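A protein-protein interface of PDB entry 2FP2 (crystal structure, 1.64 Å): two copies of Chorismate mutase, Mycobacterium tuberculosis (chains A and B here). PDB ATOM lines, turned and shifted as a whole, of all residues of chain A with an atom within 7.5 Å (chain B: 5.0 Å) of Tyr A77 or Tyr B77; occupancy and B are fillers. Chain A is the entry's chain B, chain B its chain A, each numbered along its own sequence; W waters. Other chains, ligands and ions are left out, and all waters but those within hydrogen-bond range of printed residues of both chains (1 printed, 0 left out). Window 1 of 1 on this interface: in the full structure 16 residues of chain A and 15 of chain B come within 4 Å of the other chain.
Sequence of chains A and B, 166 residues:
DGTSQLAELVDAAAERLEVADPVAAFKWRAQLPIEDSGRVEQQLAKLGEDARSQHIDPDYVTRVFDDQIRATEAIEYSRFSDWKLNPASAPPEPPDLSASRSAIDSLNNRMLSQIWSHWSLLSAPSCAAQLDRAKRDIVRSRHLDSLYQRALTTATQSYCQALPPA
The side-chain carboxylate of Glu B35 is in salt-bridge range of the side-chain amino group of Lys A84 (2.8 Å). NZ of Lys A84 is in salt-bridge range of OE1 of Glu B73 (2.8 Å). The backbone carbonyl oxygen of Ala B74 is in hydrogen-bond range of the side-chain hydroxyl of Ser A81, at 2.7 Å. The side-chain hydroxyl (OG) of Ser B81 sits at hydrogen-bond distance from the backbone carbonyl oxygen (O) of Ala A74 (2.8 Å). The side-chain carboxylate (OE2) of Glu A35 lies within salt-bridge range of the side-chain amino group (NZ) of Lys B84. O of Lys B84 lies within hydrogen-bond range of NH1 of Arg A70 (2.8 Å). The side-chain amino group (NZ) of Lys B84 is in salt-bridge range of the side-chain carboxylate (OE1) of Glu A73 (2.8 Å).
Of chain B, only Tyr B77, Phe B80, Ser B81 and Lys B84 come within 4 Å of Tyr A77. Of chain A, only Tyr A77 (3.5 Å), Phe A80 (3.6 Å) and Ser A81 (3.8 Å) come within 4 Å of Tyr B77. Of the printed residues of chain B, Arg A70 touches Lys B84 (2.8 Å). Of the printed residues of chain B, Ser A78 touches Ser B81. Of the printed residues of chain A, Ser B81 touches Ala A74 (2.8 Å), Tyr A77 (3.8 Å) and Ser A78 (3.6 Å). Of the printed residues of chain A, Glu B35 touches Phe A80 and Lys A84. Thr A72 touches none of the printed residues of chain B.
Water W1 bridges OE1 of Glu B73 (2.8 Å) and NZ of Lys A84 (3.5 Å).
Of the 23 printed residues of chain A, 9 touch a printed residue of chain B. Printed residues of chain A that touch a printed residue of chain B: Glu A35, Arg A70, Glu A73, Ala A74, Tyr A77, Ser A78, Phe A80, Ser A81 and Lys A84. Hydrophobic or aromatic side chains of chain B within 4 Å of the printed part of chain A: Ala B74, Tyr B77 and Phe B80. Among the printed residues, 18 pairs touch across the chains. Among the printed residues, Asp or Glu carboxylates within 4 Å of a Lys or Arg side-chain nitrogen of the other chain: Glu A35 with Lys B84 (3.1 Å), Glu A73 with Lys B84 (2.8 Å), Lys A84 with Glu B35 (2.8 Å) and Lys A84 with Glu B73 (2.8 Å).
Glu A35 touches Lys B84, and with the chains exchanged Lys A84 touches Glu B35. Ala A74 touches Ser B81, and with the chains exchanged Ser A81 touches Ala B74. Tyr A77 touches Ser B81, and with the chains exchanged Ser A81 touches Tyr B77. Phe A80 touches Glu B35, but with the chains exchanged Glu A35 does not touch Phe B80 (5.5 Å). 12 positions are printed for both chains.
The side-chain carboxylate (OE1) of Glu B35 is in hydrogen-bond range of the side-chain hydroxyl (OH) of Tyr B77 (2.5 Å). The side-chain carboxylate (OE1) of Glu A35 lies within hydrogen-bond range of the side-chain hydroxyl (OH) of Tyr A77 (2.7 Å).
Ala A74 touches Lys B84. Tyr A77 touches Tyr B77 (O to CB, 3.5 Å). Phe B80 touches Tyr A77 (CD2 to CZ, 3.8 Å). Tyr A77 touches Ser B81. CG of Lys B84 touches CE2 of Tyr A77, 3.8 Å away. Ser A78 touches Ser B81. CD2 of Phe A80 touches OE1 of Glu B35 (3.99 Å). CD2 of Phe A80 touches OH of Tyr B77, at 3.6 Å. Tyr B77 touches Ser A81 (CB to N, 3.8 Å). Ser B78 touches Ser A81 (CB to OG, 3.7 Å).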
ATOM      1  N   ALA A  20      -2.539 -28.321 -13.147  1.00  0.00           N
ATOM      2  CA  ALA A  20      -1.991 -27.051 -13.678  1.00  0.00           C
ATOM      3  C   ALA A  20      -2.964 -25.918 -13.443  1.00  0.00           C
ATOM      4  O   ALA A  20      -2.522 -24.777 -13.224  1.00  0.00           O
ATOM      5  CB  ALA A  20      -1.678 -27.140 -15.201  1.00  0.00           C
ATOM      6  N   ALA A  24      -1.923 -22.695 -11.459  1.00  0.00           N
ATOM      7  CA  ALA A  24      -1.906 -21.425 -12.218  1.00  0.00           C
ATOM      8  C   ALA A  24      -2.719 -20.375 -11.456  1.00  0.00           C
ATOM      9  O   ALA A  24      -2.261 -19.242 -11.279  1.00  0.00           O
ATOM     10  CB  ALA A  24      -2.462 -21.620 -13.639  1.00  0.00           C
ATOM     11  N   TRP A  28      -1.307 -16.882 -10.040  1.00  0.00           N
ATOM     12  CA  TRP A  28      -1.858 -15.674 -10.640  1.00  0.00           C
ATOM     13  C   TRP A  28      -2.187 -14.679  -9.514  1.00  0.00           C
ATOM     14  O   TRP A  28      -1.783 -13.518  -9.565  1.00  0.00           O
ATOM     15  CB  TRP A  28      -3.104 -16.016 -11.444  1.00  0.00           C
ATOM     16  CG  TRP A  28      -3.830 -14.841 -12.018  1.00  0.00           C
ATOM     17  CD1 TRP A  28      -4.895 -14.208 -11.471  1.00  0.00           C
ATOM     18  CD2 TRP A  28      -3.544 -14.163 -13.256  1.00  0.00           C
ATOM     19  NE1 TRP A  28      -5.315 -13.178 -12.293  1.00  0.00           N
ATOM     20  CE2 TRP A  28      -4.478 -13.114 -13.380  1.00  0.00           C
ATOM     21  CE3 TRP A  28      -2.569 -14.320 -14.249  1.00  0.00           C
ATOM     22  CZ2 TRP A  28      -4.495 -12.265 -14.467  1.00  0.00           C
ATOM     23  CZ3 TRP A  28      -2.589 -13.461 -15.341  1.00  0.00           C
ATOM     24  CH2 TRP A  28      -3.542 -12.443 -15.425  1.00  0.00           C
ATOM     25  N   LEU A  32       3.266 -15.084  -8.525  1.00  0.00           N
ATOM     26  CA  LEU A  32       4.437 -15.949  -8.521  1.00  0.00           C
ATOM     27  C   LEU A  32       4.760 -16.375  -9.957  1.00  0.00           C
ATOM     28  O   LEU A  32       3.850 -16.533 -10.771  1.00  0.00           O
ATOM     29  CB  LEU A  32       4.195 -17.191  -7.680  1.00  0.00           C
ATOM     30  CG  LEU A  32       3.923 -17.031  -6.174  1.00  0.00           C
ATOM     31  CD1 LEU A  32       3.218 -18.248  -5.640  1.00  0.00           C
ATOM     32  CD2 LEU A  32       5.251 -16.769  -5.453  1.00  0.00           C
ATOM     33  N   PRO A  33       6.060 -16.548 -10.268  1.00  0.00           N
ATOM     34  CA  PRO A  33       6.404 -17.131 -11.562  1.00  0.00           C
ATOM     35  C   PRO A  33       5.798 -18.520 -11.779  1.00  0.00           C
ATOM     36  O   PRO A  33       5.526 -19.252 -10.823  1.00  0.00           O
ATOM     37  CB  PRO A  33       7.934 -17.253 -11.507  1.00  0.00           C
ATOM     38  CG  PRO A  33       8.382 -16.301 -10.462  1.00  0.00           C
ATOM     39  CD  PRO A  33       7.252 -16.180  -9.482  1.00  0.00           C
ATOM     40  N   ILE A  34       5.650 -18.882 -13.042  1.00  0.00           N
ATOM     41  CA  ILE A  34       5.128 -20.200 -13.410  1.00  0.00           C
ATOM     42  C   ILE A  34       6.187 -21.260 -13.213  1.00  0.00           C
ATOM     43  O   ILE A  34       5.902 -22.322 -12.657  1.00  0.00           O
ATOM     44  CB  ILE A  34       4.618 -20.213 -14.866  1.00  0.00           C
ATOM     45  CG1 ILE A  34       3.222 -19.563 -14.888  1.00  0.00           C
ATOM     46  CG2 ILE A  34       4.503 -21.637 -15.431  1.00  0.00           C
ATOM     47  CD1 ILE A  34       2.811 -19.084 -16.199  1.00  0.00           C
ATOM     48  N   GLU A  35       7.397 -20.991 -13.690  1.00  0.00           N
ATOM     49  CA  GLU A  35       8.485 -21.953 -13.554  1.00  0.00           C
ATOM     50  C   GLU A  35       9.136 -21.848 -12.172  1.00  0.00           C
ATOM     51  O   GLU A  35       9.445 -20.754 -11.683  1.00  0.00           O
ATOM     52  CB  GLU A  35       9.482 -21.811 -14.694  1.00  0.00           C
ATOM     53  CG  GLU A  35       8.820 -22.108 -16.011  1.00  0.00           C
ATOM     54  CD  GLU A  35       9.774 -22.162 -17.168  1.00  0.00           C
ATOM     55  OE1 GLU A  35       9.433 -21.608 -18.236  1.00  0.00           O
ATOM     56  OE2 GLU A  35      10.868 -22.760 -17.013  1.00  0.00           O
ATOM     57  N   ARG A  70       7.110 -30.056 -18.339  1.00  0.00           N
ATOM     58  CA  ARG A  70       7.040 -29.048 -19.412  1.00  0.00           C
ATOM     59  C   ARG A  70       5.588 -28.842 -19.895  1.00  0.00           C
ATOM     60  O   ARG A  70       5.088 -27.723 -20.092  1.00  0.00           O
ATOM     61  CB  ARG A  70       7.973 -29.485 -20.542  1.00  0.00           C
ATOM     62  CG  ARG A  70       8.204 -28.465 -21.566  1.00  0.00           C
ATOM     63  CD  ARG A  70       9.499 -28.748 -22.363  1.00  0.00           C
ATOM     64  NE  ARG A  70       9.623 -30.169 -22.673  1.00  0.00           N
ATOM     65  CZ  ARG A  70       9.068 -30.797 -23.706  1.00  0.00           C
ATOM     66  NH1 ARG A  70       8.353 -30.161 -24.634  1.00  0.00           N
ATOM     67  NH2 ARG A  70       9.266 -32.098 -23.853  1.00  0.00           N
ATOM     68  N   ALA A  71       4.861 -29.945 -20.076  1.00  0.00           N
ATOM     69  CA  ALA A  71       3.472 -29.861 -20.474  1.00  0.00           C
ATOM     70  C   ALA A  71       2.609 -29.089 -19.463  1.00  0.00           C
ATOM     71  O   ALA A  71       1.660 -28.368 -19.831  1.00  0.00           O
ATOM     72  CB  ALA A  71       2.925 -31.275 -20.698  1.00  0.00           C
ATOM     73  N   THR A  72       2.935 -29.283 -18.196  1.00  0.00           N
ATOM     74  CA  THR A  72       2.217 -28.650 -17.089  1.00  0.00           C
ATOM     75  C   THR A  72       2.465 -27.149 -17.145  1.00  0.00           C
ATOM     76  O   THR A  72       1.532 -26.364 -17.067  1.00  0.00           O
ATOM     77  CB  THR A  72       2.659 -29.255 -15.750  1.00  0.00           C
ATOM     78  OG1 THR A  72       2.471 -30.692 -15.819  1.00  0.00           O
ATOM     79  CG2 THR A  72       1.812 -28.723 -14.569  1.00  0.00           C
ATOM     80  N   GLU A  73       3.724 -26.794 -17.294  1.00  0.00           N
ATOM     81  CA  GLU A  73       4.103 -25.370 -17.445  1.00  0.00           C
ATOM     82  C   GLU A  73       3.408 -24.760 -18.653  1.00  0.00           C
ATOM     83  O   GLU A  73       2.915 -23.621 -18.595  1.00  0.00           O
ATOM     84  CB  GLU A  73       5.613 -25.212 -17.514  1.00  0.00           C
ATOM     85  CG  GLU A  73       6.292 -25.581 -16.245  1.00  0.00           C
ATOM     86  CD  GLU A  73       7.777 -25.832 -16.319  1.00  0.00           C
ATOM     87  OE1 GLU A  73       8.356 -25.978 -17.408  1.00  0.00           O
ATOM     88  OE2 GLU A  73       8.361 -25.930 -15.228  1.00  0.00           O
ATOM     89  N   ALA A  74       3.337 -25.505 -19.763  1.00  0.00           N
ATOM     90  CA  ALA A  74       2.601 -25.014 -20.920  1.00  0.00           C
ATOM     91  C   ALA A  74       1.137 -24.656 -20.626  1.00  0.00           C
ATOM     92  O   ALA A  74       0.614 -23.616 -21.065  1.00  0.00           O
ATOM     93  CB  ALA A  74       2.673 -26.029 -22.068  1.00  0.00           C
ATOM     94  N   ILE A  75       0.437 -25.512 -19.881  1.00  0.00           N
ATOM     95  CA  ILE A  75      -0.930 -25.236 -19.509  1.00  0.00           C
ATOM     96  C   ILE A  75      -0.998 -23.972 -18.624  1.00  0.00           C
ATOM     97  O   ILE A  75      -1.851 -23.105 -18.866  1.00  0.00           O
ATOM     98  CB  ILE A  75      -1.585 -26.432 -18.794  1.00  0.00           C
ATOM     99  CG1 ILE A  75      -1.755 -27.585 -19.782  1.00  0.00           C
ATOM    100  CG2 ILE A  75      -2.899 -25.994 -18.183  1.00  0.00           C
ATOM    101  CD1 ILE A  75      -2.055 -28.929 -19.058  1.00  0.00           C
ATOM    102  N   GLU A  76      -0.106 -23.876 -17.647  1.00  0.00           N
ATOM    103  CA  GLU A  76      -0.079 -22.686 -16.753  1.00  0.00           C
ATOM    104  C   GLU A  76       0.111 -21.398 -17.571  1.00  0.00           C
ATOM    105  O   GLU A  76      -0.658 -20.443 -17.391  1.00  0.00           O
ATOM    106  CB  GLU A  76       0.981 -22.814 -15.702  1.00  0.00           C
ATOM    107  CG  GLU A  76       0.741 -23.971 -14.755  1.00  0.00           C
ATOM    108  CD  GLU A  76       1.807 -24.125 -13.709  1.00  0.00           C
ATOM    109  OE1 GLU A  76       2.195 -23.123 -13.067  1.00  0.00           O
ATOM    110  OE2 GLU A  76       2.261 -25.291 -13.493  1.00  0.00           O
ATOM    111  N   TYR A  77       1.047 -21.413 -18.524  1.00  0.00           N
ATOM    112  CA  TYR A  77       1.226 -20.242 -19.431  1.00  0.00           C
ATOM    113  C   TYR A  77      -0.015 -19.914 -20.228  1.00  0.00           C
ATOM    114  O   TYR A  77      -0.393 -18.739 -20.401  1.00  0.00           O
ATOM    115  CB  TYR A  77       2.376 -20.453 -20.391  1.00  0.00           C
ATOM    116  CG  TYR A  77       3.759 -20.270 -19.800  1.00  0.00           C
ATOM    117  CD1 TYR A  77       4.088 -19.130 -19.079  1.00  0.00           C
ATOM    118  CD2 TYR A  77       4.731 -21.245 -19.952  1.00  0.00           C
ATOM    119  CE1 TYR A  77       5.349 -18.962 -18.546  1.00  0.00           C
ATOM    120  CE2 TYR A  77       6.017 -21.072 -19.425  1.00  0.00           C
ATOM    121  CZ  TYR A  77       6.304 -19.929 -18.702  1.00  0.00           C
ATOM    122  OH  TYR A  77       7.569 -19.698 -18.165  1.00  0.00           O
ATOM    123  N   SER A  78      -0.685 -20.936 -20.753  1.00  0.00           N
ATOM    124  CA  SER A  78      -1.907 -20.702 -21.480  1.00  0.00           C
ATOM    125  C   SER A  78      -2.991 -20.064 -20.608  1.00  0.00           C
ATOM    126  O   SER A  78      -3.732 -19.186 -21.046  1.00  0.00           O
ATOM    127  CB  SER A  78      -2.402 -22.031 -22.100  1.00  0.00           C
ATOM    128  OG  SER A  78      -3.550 -21.821 -22.893  1.00  0.00           O
ATOM    129  N   ARG A  79      -3.137 -20.553 -19.377  1.00  0.00           N
ATOM    130  CA  ARG A  79      -4.150 -19.947 -18.481  1.00  0.00           C
ATOM    131  C   ARG A  79      -3.820 -18.468 -18.171  1.00  0.00           C
ATOM    132  O   ARG A  79      -4.710 -17.601 -18.185  1.00  0.00           O
ATOM    133  CB  ARG A  79      -4.300 -20.732 -17.192  1.00  0.00           C
ATOM    134  CG  ARG A  79      -4.857 -22.124 -17.377  1.00  0.00           C
ATOM    135  CD  ARG A  79      -6.000 -22.190 -18.311  1.00  0.00           C
ATOM    136  NE  ARG A  79      -6.733 -23.454 -18.105  1.00  0.00           N
ATOM    137  CZ  ARG A  79      -7.404 -24.134 -19.041  1.00  0.00           C
ATOM    138  NH1 ARG A  79      -7.437 -23.732 -20.314  1.00  0.00           N
ATOM    139  NH2 ARG A  79      -8.077 -25.236 -18.692  1.00  0.00           N
ATOM    140  N   PHE A  80      -2.539 -18.186 -17.915  1.00  0.00           N
ATOM    141  CA  PHE A  80      -2.110 -16.784 -17.735  1.00  0.00           C
ATOM    142  C   PHE A  80      -2.478 -15.936 -18.977  1.00  0.00           C
ATOM    143  O   PHE A  80      -2.940 -14.809 -18.869  1.00  0.00           O
ATOM    144  CB  PHE A  80      -0.631 -16.717 -17.438  1.00  0.00           C
ATOM    145  CG  PHE A  80      -0.289 -16.807 -15.965  1.00  0.00           C
ATOM    146  CD1 PHE A  80      -0.878 -17.734 -15.126  1.00  0.00           C
ATOM    147  CD2 PHE A  80       0.621 -15.918 -15.401  1.00  0.00           C
ATOM    148  CE1 PHE A  80      -0.538 -17.778 -13.764  1.00  0.00           C
ATOM    149  CE2 PHE A  80       0.965 -15.964 -14.033  1.00  0.00           C
ATOM    150  CZ  PHE A  80       0.385 -16.877 -13.226  1.00  0.00           C
ATOM    151  N   SER A  81      -2.282 -16.501 -20.158  1.00  0.00           N
ATOM    152  CA  SER A  81      -2.705 -15.813 -21.385  1.00  0.00           C
ATOM    153  C   SER A  81      -4.213 -15.489 -21.330  1.00  0.00           C
ATOM    154  O   SER A  81      -4.637 -14.367 -21.566  1.00  0.00           O
ATOM    155  CB  SER A  81      -2.388 -16.662 -22.606  1.00  0.00           C
ATOM    156  OG  SER A  81      -2.841 -16.047 -23.781  1.00  0.00           O
ATOM    157  N   ASP A  82      -5.028 -16.517 -21.079  1.00  0.00           N
ATOM    158  CA  ASP A  82      -6.459 -16.326 -20.959  1.00  0.00           C
ATOM    159  C   ASP A  82      -6.838 -15.247 -19.930  1.00  0.00           C
ATOM    160  O   ASP A  82      -7.767 -14.462 -20.184  1.00  0.00           O
ATOM    161  CB  ASP A  82      -7.145 -17.642 -20.547  1.00  0.00           C
ATOM    162  CG  ASP A  82      -7.096 -18.712 -21.610  1.00  0.00           C
ATOM    163  OD1 ASP A  82      -6.812 -18.467 -22.799  1.00  0.00           O
ATOM    164  OD2 ASP A  82      -7.291 -19.890 -21.183  1.00  0.00           O
ATOM    165  N   TRP A  83      -6.155 -15.226 -18.786  1.00  0.00           N
ATOM    166  CA  TRP A  83      -6.507 -14.346 -17.672  1.00  0.00           C
ATOM    167  C   TRP A  83      -5.991 -12.958 -17.921  1.00  0.00           C
ATOM    168  O   TRP A  83      -6.583 -11.991 -17.442  1.00  0.00           O
ATOM    169  CB  TRP A  83      -6.045 -14.912 -16.359  1.00  0.00           C
ATOM    170  CG  TRP A  83      -6.689 -16.255 -16.063  1.00  0.00           C
ATOM    171  CD1 TRP A  83      -7.897 -16.698 -16.484  1.00  0.00           C
ATOM    172  CD2 TRP A  83      -6.129 -17.307 -15.259  1.00  0.00           C
ATOM    173  NE1 TRP A  83      -8.138 -17.993 -15.989  1.00  0.00           N
ATOM    174  CE2 TRP A  83      -7.060 -18.376 -15.246  1.00  0.00           C
ATOM    175  CE3 TRP A  83      -4.936 -17.466 -14.591  1.00  0.00           C
ATOM    176  CZ2 TRP A  83      -6.810 -19.586 -14.522  1.00  0.00           C
ATOM    177  CZ3 TRP A  83      -4.690 -18.669 -13.865  1.00  0.00           C
ATOM    178  CH2 TRP A  83      -5.628 -19.699 -13.865  1.00  0.00           C
ATOM    179  N   LYS A  84      -4.902 -12.828 -18.669  1.00  0.00           N
ATOM    180  CA  LYS A  84      -4.524 -11.492 -19.134  1.00  0.00           C
ATOM    181  C   LYS A  84      -5.606 -10.900 -20.052  1.00  0.00           C
ATOM    182  O   LYS A  84      -5.824  -9.679 -20.050  1.00  0.00           O
ATOM    183  CB  LYS A  84      -3.172 -11.524 -19.827  1.00  0.00           C
ATOM    184  CG  LYS A  84      -2.007 -11.605 -18.893  1.00  0.00           C
ATOM    185  CD  LYS A  84      -1.658 -10.285 -18.169  1.00  0.00           C
ATOM    186  CE  LYS A  84      -0.557 -10.435 -17.205  1.00  0.00           C
ATOM    187  NZ  LYS A  84      -0.291  -9.123 -16.508  1.00  0.00           N
ATOM    188  N   LEU A 147      -6.053 -27.766 -25.816  1.00  0.00           N
ATOM    189  CA  LEU A 147      -4.828 -27.504 -25.077  1.00  0.00           C
ATOM    190  C   LEU A 147      -4.385 -28.780 -24.346  1.00  0.00           C
ATOM    191  O   LEU A 147      -3.215 -29.168 -24.401  1.00  0.00           O
ATOM    192  CB  LEU A 147      -5.049 -26.392 -24.035  1.00  0.00           C
ATOM    193  CG  LEU A 147      -3.897 -26.109 -23.061  1.00  0.00           C
ATOM    194  CD1 LEU A 147      -2.622 -25.630 -23.781  1.00  0.00           C
ATOM    195  CD2 LEU A 147      -4.370 -25.115 -22.069  1.00  0.00           C
ATOM    196  N   ILE B  34       7.886 -12.924 -18.811  1.00  0.00           N
ATOM    197  CA  ILE B  34       6.986 -12.057 -19.580  1.00  0.00           C
ATOM    198  C   ILE B  34       6.676 -10.771 -18.821  1.00  0.00           C
ATOM    199  O   ILE B  34       6.840  -9.676 -19.340  1.00  0.00           O
ATOM    200  CB  ILE B  34       5.656 -12.759 -19.889  1.00  0.00           C
ATOM    201  CG1 ILE B  34       5.868 -13.967 -20.813  1.00  0.00           C
ATOM    202  CG2 ILE B  34       4.630 -11.762 -20.486  1.00  0.00           C
ATOM    203  CD1 ILE B  34       6.751 -13.694 -22.029  1.00  0.00           C
ATOM    204  N   GLU B  35       6.182 -10.941 -17.607  1.00  0.00           N
ATOM    205  CA  GLU B  35       5.690  -9.806 -16.824  1.00  0.00           C
ATOM    206  C   GLU B  35       6.761  -9.129 -16.012  1.00  0.00           C
ATOM    207  O   GLU B  35       7.824  -9.689 -15.674  1.00  0.00           O
ATOM    208  CB  GLU B  35       4.567 -10.226 -15.892  1.00  0.00           C
ATOM    209  CG  GLU B  35       3.277 -10.634 -16.531  1.00  0.00           C
ATOM    210  CD  GLU B  35       2.230 -10.953 -15.510  1.00  0.00           C
ATOM    211  OE1 GLU B  35       1.923 -12.144 -15.287  1.00  0.00           O
ATOM    212  OE2 GLU B  35       1.736  -9.989 -14.857  1.00  0.00           O
ATOM    213  N   GLU B  73       0.807  -8.975 -23.315  1.00  0.00           N
ATOM    214  CA  GLU B  73       1.344 -10.013 -22.423  1.00  0.00           C
ATOM    215  C   GLU B  73       0.590 -11.324 -22.670  1.00  0.00           C
ATOM    216  O   GLU B  73       1.183 -12.401 -22.677  1.00  0.00           O
ATOM    217  CB  GLU B  73       1.243  -9.558 -20.980  1.00  0.00           C
ATOM    218  CG  GLU B  73       2.189  -8.413 -20.661  1.00  0.00           C
ATOM    219  CD  GLU B  73       1.998  -7.823 -19.293  1.00  0.00           C
ATOM    220  OE1 GLU B  73       0.867  -7.872 -18.761  1.00  0.00           O
ATOM    221  OE2 GLU B  73       2.973  -7.269 -18.749  1.00  0.00           O
ATOM    222  N   ALA B  74      -0.702 -11.221 -22.916  1.00  0.00           N
ATOM    223  CA  ALA B  74      -1.497 -12.437 -23.239  1.00  0.00           C
ATOM    224  C   ALA B  74      -0.916 -13.151 -24.451  1.00  0.00           C
ATOM    225  O   ALA B  74      -0.794 -14.391 -24.457  1.00  0.00           O
ATOM    226  CB  ALA B  74      -2.955 -12.096 -23.501  1.00  0.00           C
ATOM    227  N   ILE B  75      -0.543 -12.409 -25.479  1.00  0.00           N
ATOM    228  CA  ILE B  75       0.030 -13.059 -26.674  1.00  0.00           C
ATOM    229  C   ILE B  75       1.365 -13.715 -26.313  1.00  0.00           C
ATOM    230  O   ILE B  75       1.650 -14.844 -26.733  1.00  0.00           O
ATOM    231  CB  ILE B  75       0.169 -12.037 -27.836  1.00  0.00           C
ATOM    232  CG1 ILE B  75      -1.201 -11.561 -28.309  1.00  0.00           C
ATOM    233  CG2 ILE B  75       0.906 -12.661 -29.075  1.00  0.00           C
ATOM    234  CD1 ILE B  75      -1.145 -10.276 -29.106  1.00  0.00           C
ATOM    235  N   GLU B  76       2.221 -12.981 -25.605  1.00  0.00           N
ATOM    236  CA  GLU B  76       3.523 -13.509 -25.170  1.00  0.00           C
ATOM    237  C   GLU B  76       3.356 -14.811 -24.390  1.00  0.00           C
ATOM    238  O   GLU B  76       4.099 -15.784 -24.642  1.00  0.00           O
ATOM    239  CB  GLU B  76       4.279 -12.483 -24.358  1.00  0.00           C
ATOM    240  CG  GLU B  76       4.519 -11.171 -25.138  1.00  0.00           C
ATOM    241  CD  GLU B  76       5.225 -10.124 -24.323  1.00  0.00           C
ATOM    242  OE1 GLU B  76       6.217 -10.435 -23.657  1.00  0.00           O
ATOM    243  OE2 GLU B  76       4.777  -8.932 -24.369  1.00  0.00           O
ATOM    244  N   TYR B  77       2.396 -14.859 -23.467  1.00  0.00           N
ATOM    245  CA  TYR B  77       2.165 -16.079 -22.657  1.00  0.00           C
ATOM    246  C   TYR B  77       1.692 -17.229 -23.537  1.00  0.00           C
ATOM    247  O   TYR B  77       2.093 -18.392 -23.317  1.00  0.00           O
ATOM    248  CB  TYR B  77       1.146 -15.808 -21.574  1.00  0.00           C
ATOM    249  CG  TYR B  77       1.719 -15.241 -20.302  1.00  0.00           C
ATOM    250  CD1 TYR B  77       2.760 -15.884 -19.639  1.00  0.00           C
ATOM    251  CD2 TYR B  77       1.189 -14.089 -19.728  1.00  0.00           C
ATOM    252  CE1 TYR B  77       3.271 -15.409 -18.423  1.00  0.00           C
ATOM    253  CE2 TYR B  77       1.694 -13.610 -18.532  1.00  0.00           C
ATOM    254  CZ  TYR B  77       2.736 -14.268 -17.882  1.00  0.00           C
ATOM    255  OH  TYR B  77       3.234 -13.815 -16.646  1.00  0.00           O
ATOM    256  N   SER B  78       0.858 -16.912 -24.533  1.00  0.00           N
ATOM    257  CA  SER B  78       0.369 -17.962 -25.443  1.00  0.00           C
ATOM    258  C   SER B  78       1.545 -18.573 -26.211  1.00  0.00           C
ATOM    259  O   SER B  78       1.645 -19.781 -26.382  1.00  0.00           O
ATOM    260  CB  SER B  78      -0.679 -17.412 -26.390  1.00  0.00           C
ATOM    261  OG  SER B  78      -1.156 -18.458 -27.217  1.00  0.00           O
ATOM    262  N   ARG B  79       2.439 -17.724 -26.696  1.00  0.00           N
ATOM    263  CA  ARG B  79       3.665 -18.231 -27.334  1.00  0.00           C
ATOM    264  C   ARG B  79       4.505 -19.086 -26.396  1.00  0.00           C
ATOM    265  O   ARG B  79       4.981 -20.161 -26.808  1.00  0.00           O
ATOM    266  CB  ARG B  79       4.516 -17.107 -27.864  1.00  0.00           C
ATOM    267  CG  ARG B  79       3.914 -16.213 -28.916  1.00  0.00           C
ATOM    268  CD  ARG B  79       3.064 -16.893 -29.915  1.00  0.00           C
ATOM    269  NE  ARG B  79       2.685 -16.009 -31.034  1.00  0.00           N
ATOM    270  CZ  ARG B  79       1.609 -16.139 -31.799  1.00  0.00           C
ATOM    271  NH1 ARG B  79       0.706 -17.094 -31.593  1.00  0.00           N
ATOM    272  NH2 ARG B  79       1.438 -15.299 -32.825  1.00  0.00           N
ATOM    273  N   PHE B  80       4.738 -18.635 -25.158  1.00  0.00           N
ATOM    274  CA  PHE B  80       5.486 -19.442 -24.199  1.00  0.00           C
ATOM    275  C   PHE B  80       4.854 -20.819 -24.008  1.00  0.00           C
ATOM    276  O   PHE B  80       5.564 -21.813 -23.877  1.00  0.00           O
ATOM    277  CB  PHE B  80       5.628 -18.728 -22.856  1.00  0.00           C
ATOM    278  CG  PHE B  80       6.850 -17.852 -22.763  1.00  0.00           C
ATOM    279  CD1 PHE B  80       7.298 -17.133 -23.850  1.00  0.00           C
ATOM    280  CD2 PHE B  80       7.530 -17.725 -21.555  1.00  0.00           C
ATOM    281  CE1 PHE B  80       8.412 -16.295 -23.731  1.00  0.00           C
ATOM    282  CE2 PHE B  80       8.667 -16.901 -21.444  1.00  0.00           C
ATOM    283  CZ  PHE B  80       9.074 -16.195 -22.538  1.00  0.00           C
ATOM    284  N   SER B  81       3.530 -20.851 -23.984  1.00  0.00           N
ATOM    285  CA  SER B  81       2.825 -22.128 -23.895  1.00  0.00           C
ATOM    286  C   SER B  81       3.166 -23.045 -25.055  1.00  0.00           C
ATOM    287  O   SER B  81       3.513 -24.219 -24.870  1.00  0.00           O
ATOM    288  CB  SER B  81       1.335 -21.898 -23.831  1.00  0.00           C
ATOM    289  OG  SER B  81       0.561 -23.089 -23.789  1.00  0.00           O
ATOM    290  N   LYS B  84       6.797 -24.229 -24.877  1.00  0.00           N
ATOM    291  CA  LYS B  84       7.005 -25.268 -23.878  1.00  0.00           C
ATOM    292  C   LYS B  84       6.654 -26.622 -24.483  1.00  0.00           C
ATOM    293  O   LYS B  84       7.354 -27.623 -24.251  1.00  0.00           O
ATOM    294  CB  LYS B  84       6.154 -25.023 -22.631  1.00  0.00           C
ATOM    295  CG  LYS B  84       6.780 -24.131 -21.628  1.00  0.00           C
ATOM    296  CD  LYS B  84       7.937 -24.838 -20.921  1.00  0.00           C
ATOM    297  CE  LYS B  84       8.654 -23.906 -20.005  1.00  0.00           C
ATOM    298  NZ  LYS B  84       9.813 -24.573 -19.330  1.00  0.00           N
HETATM  299  O   HOH W   1       0.330  -5.759 -17.012  1.00  0.00           O
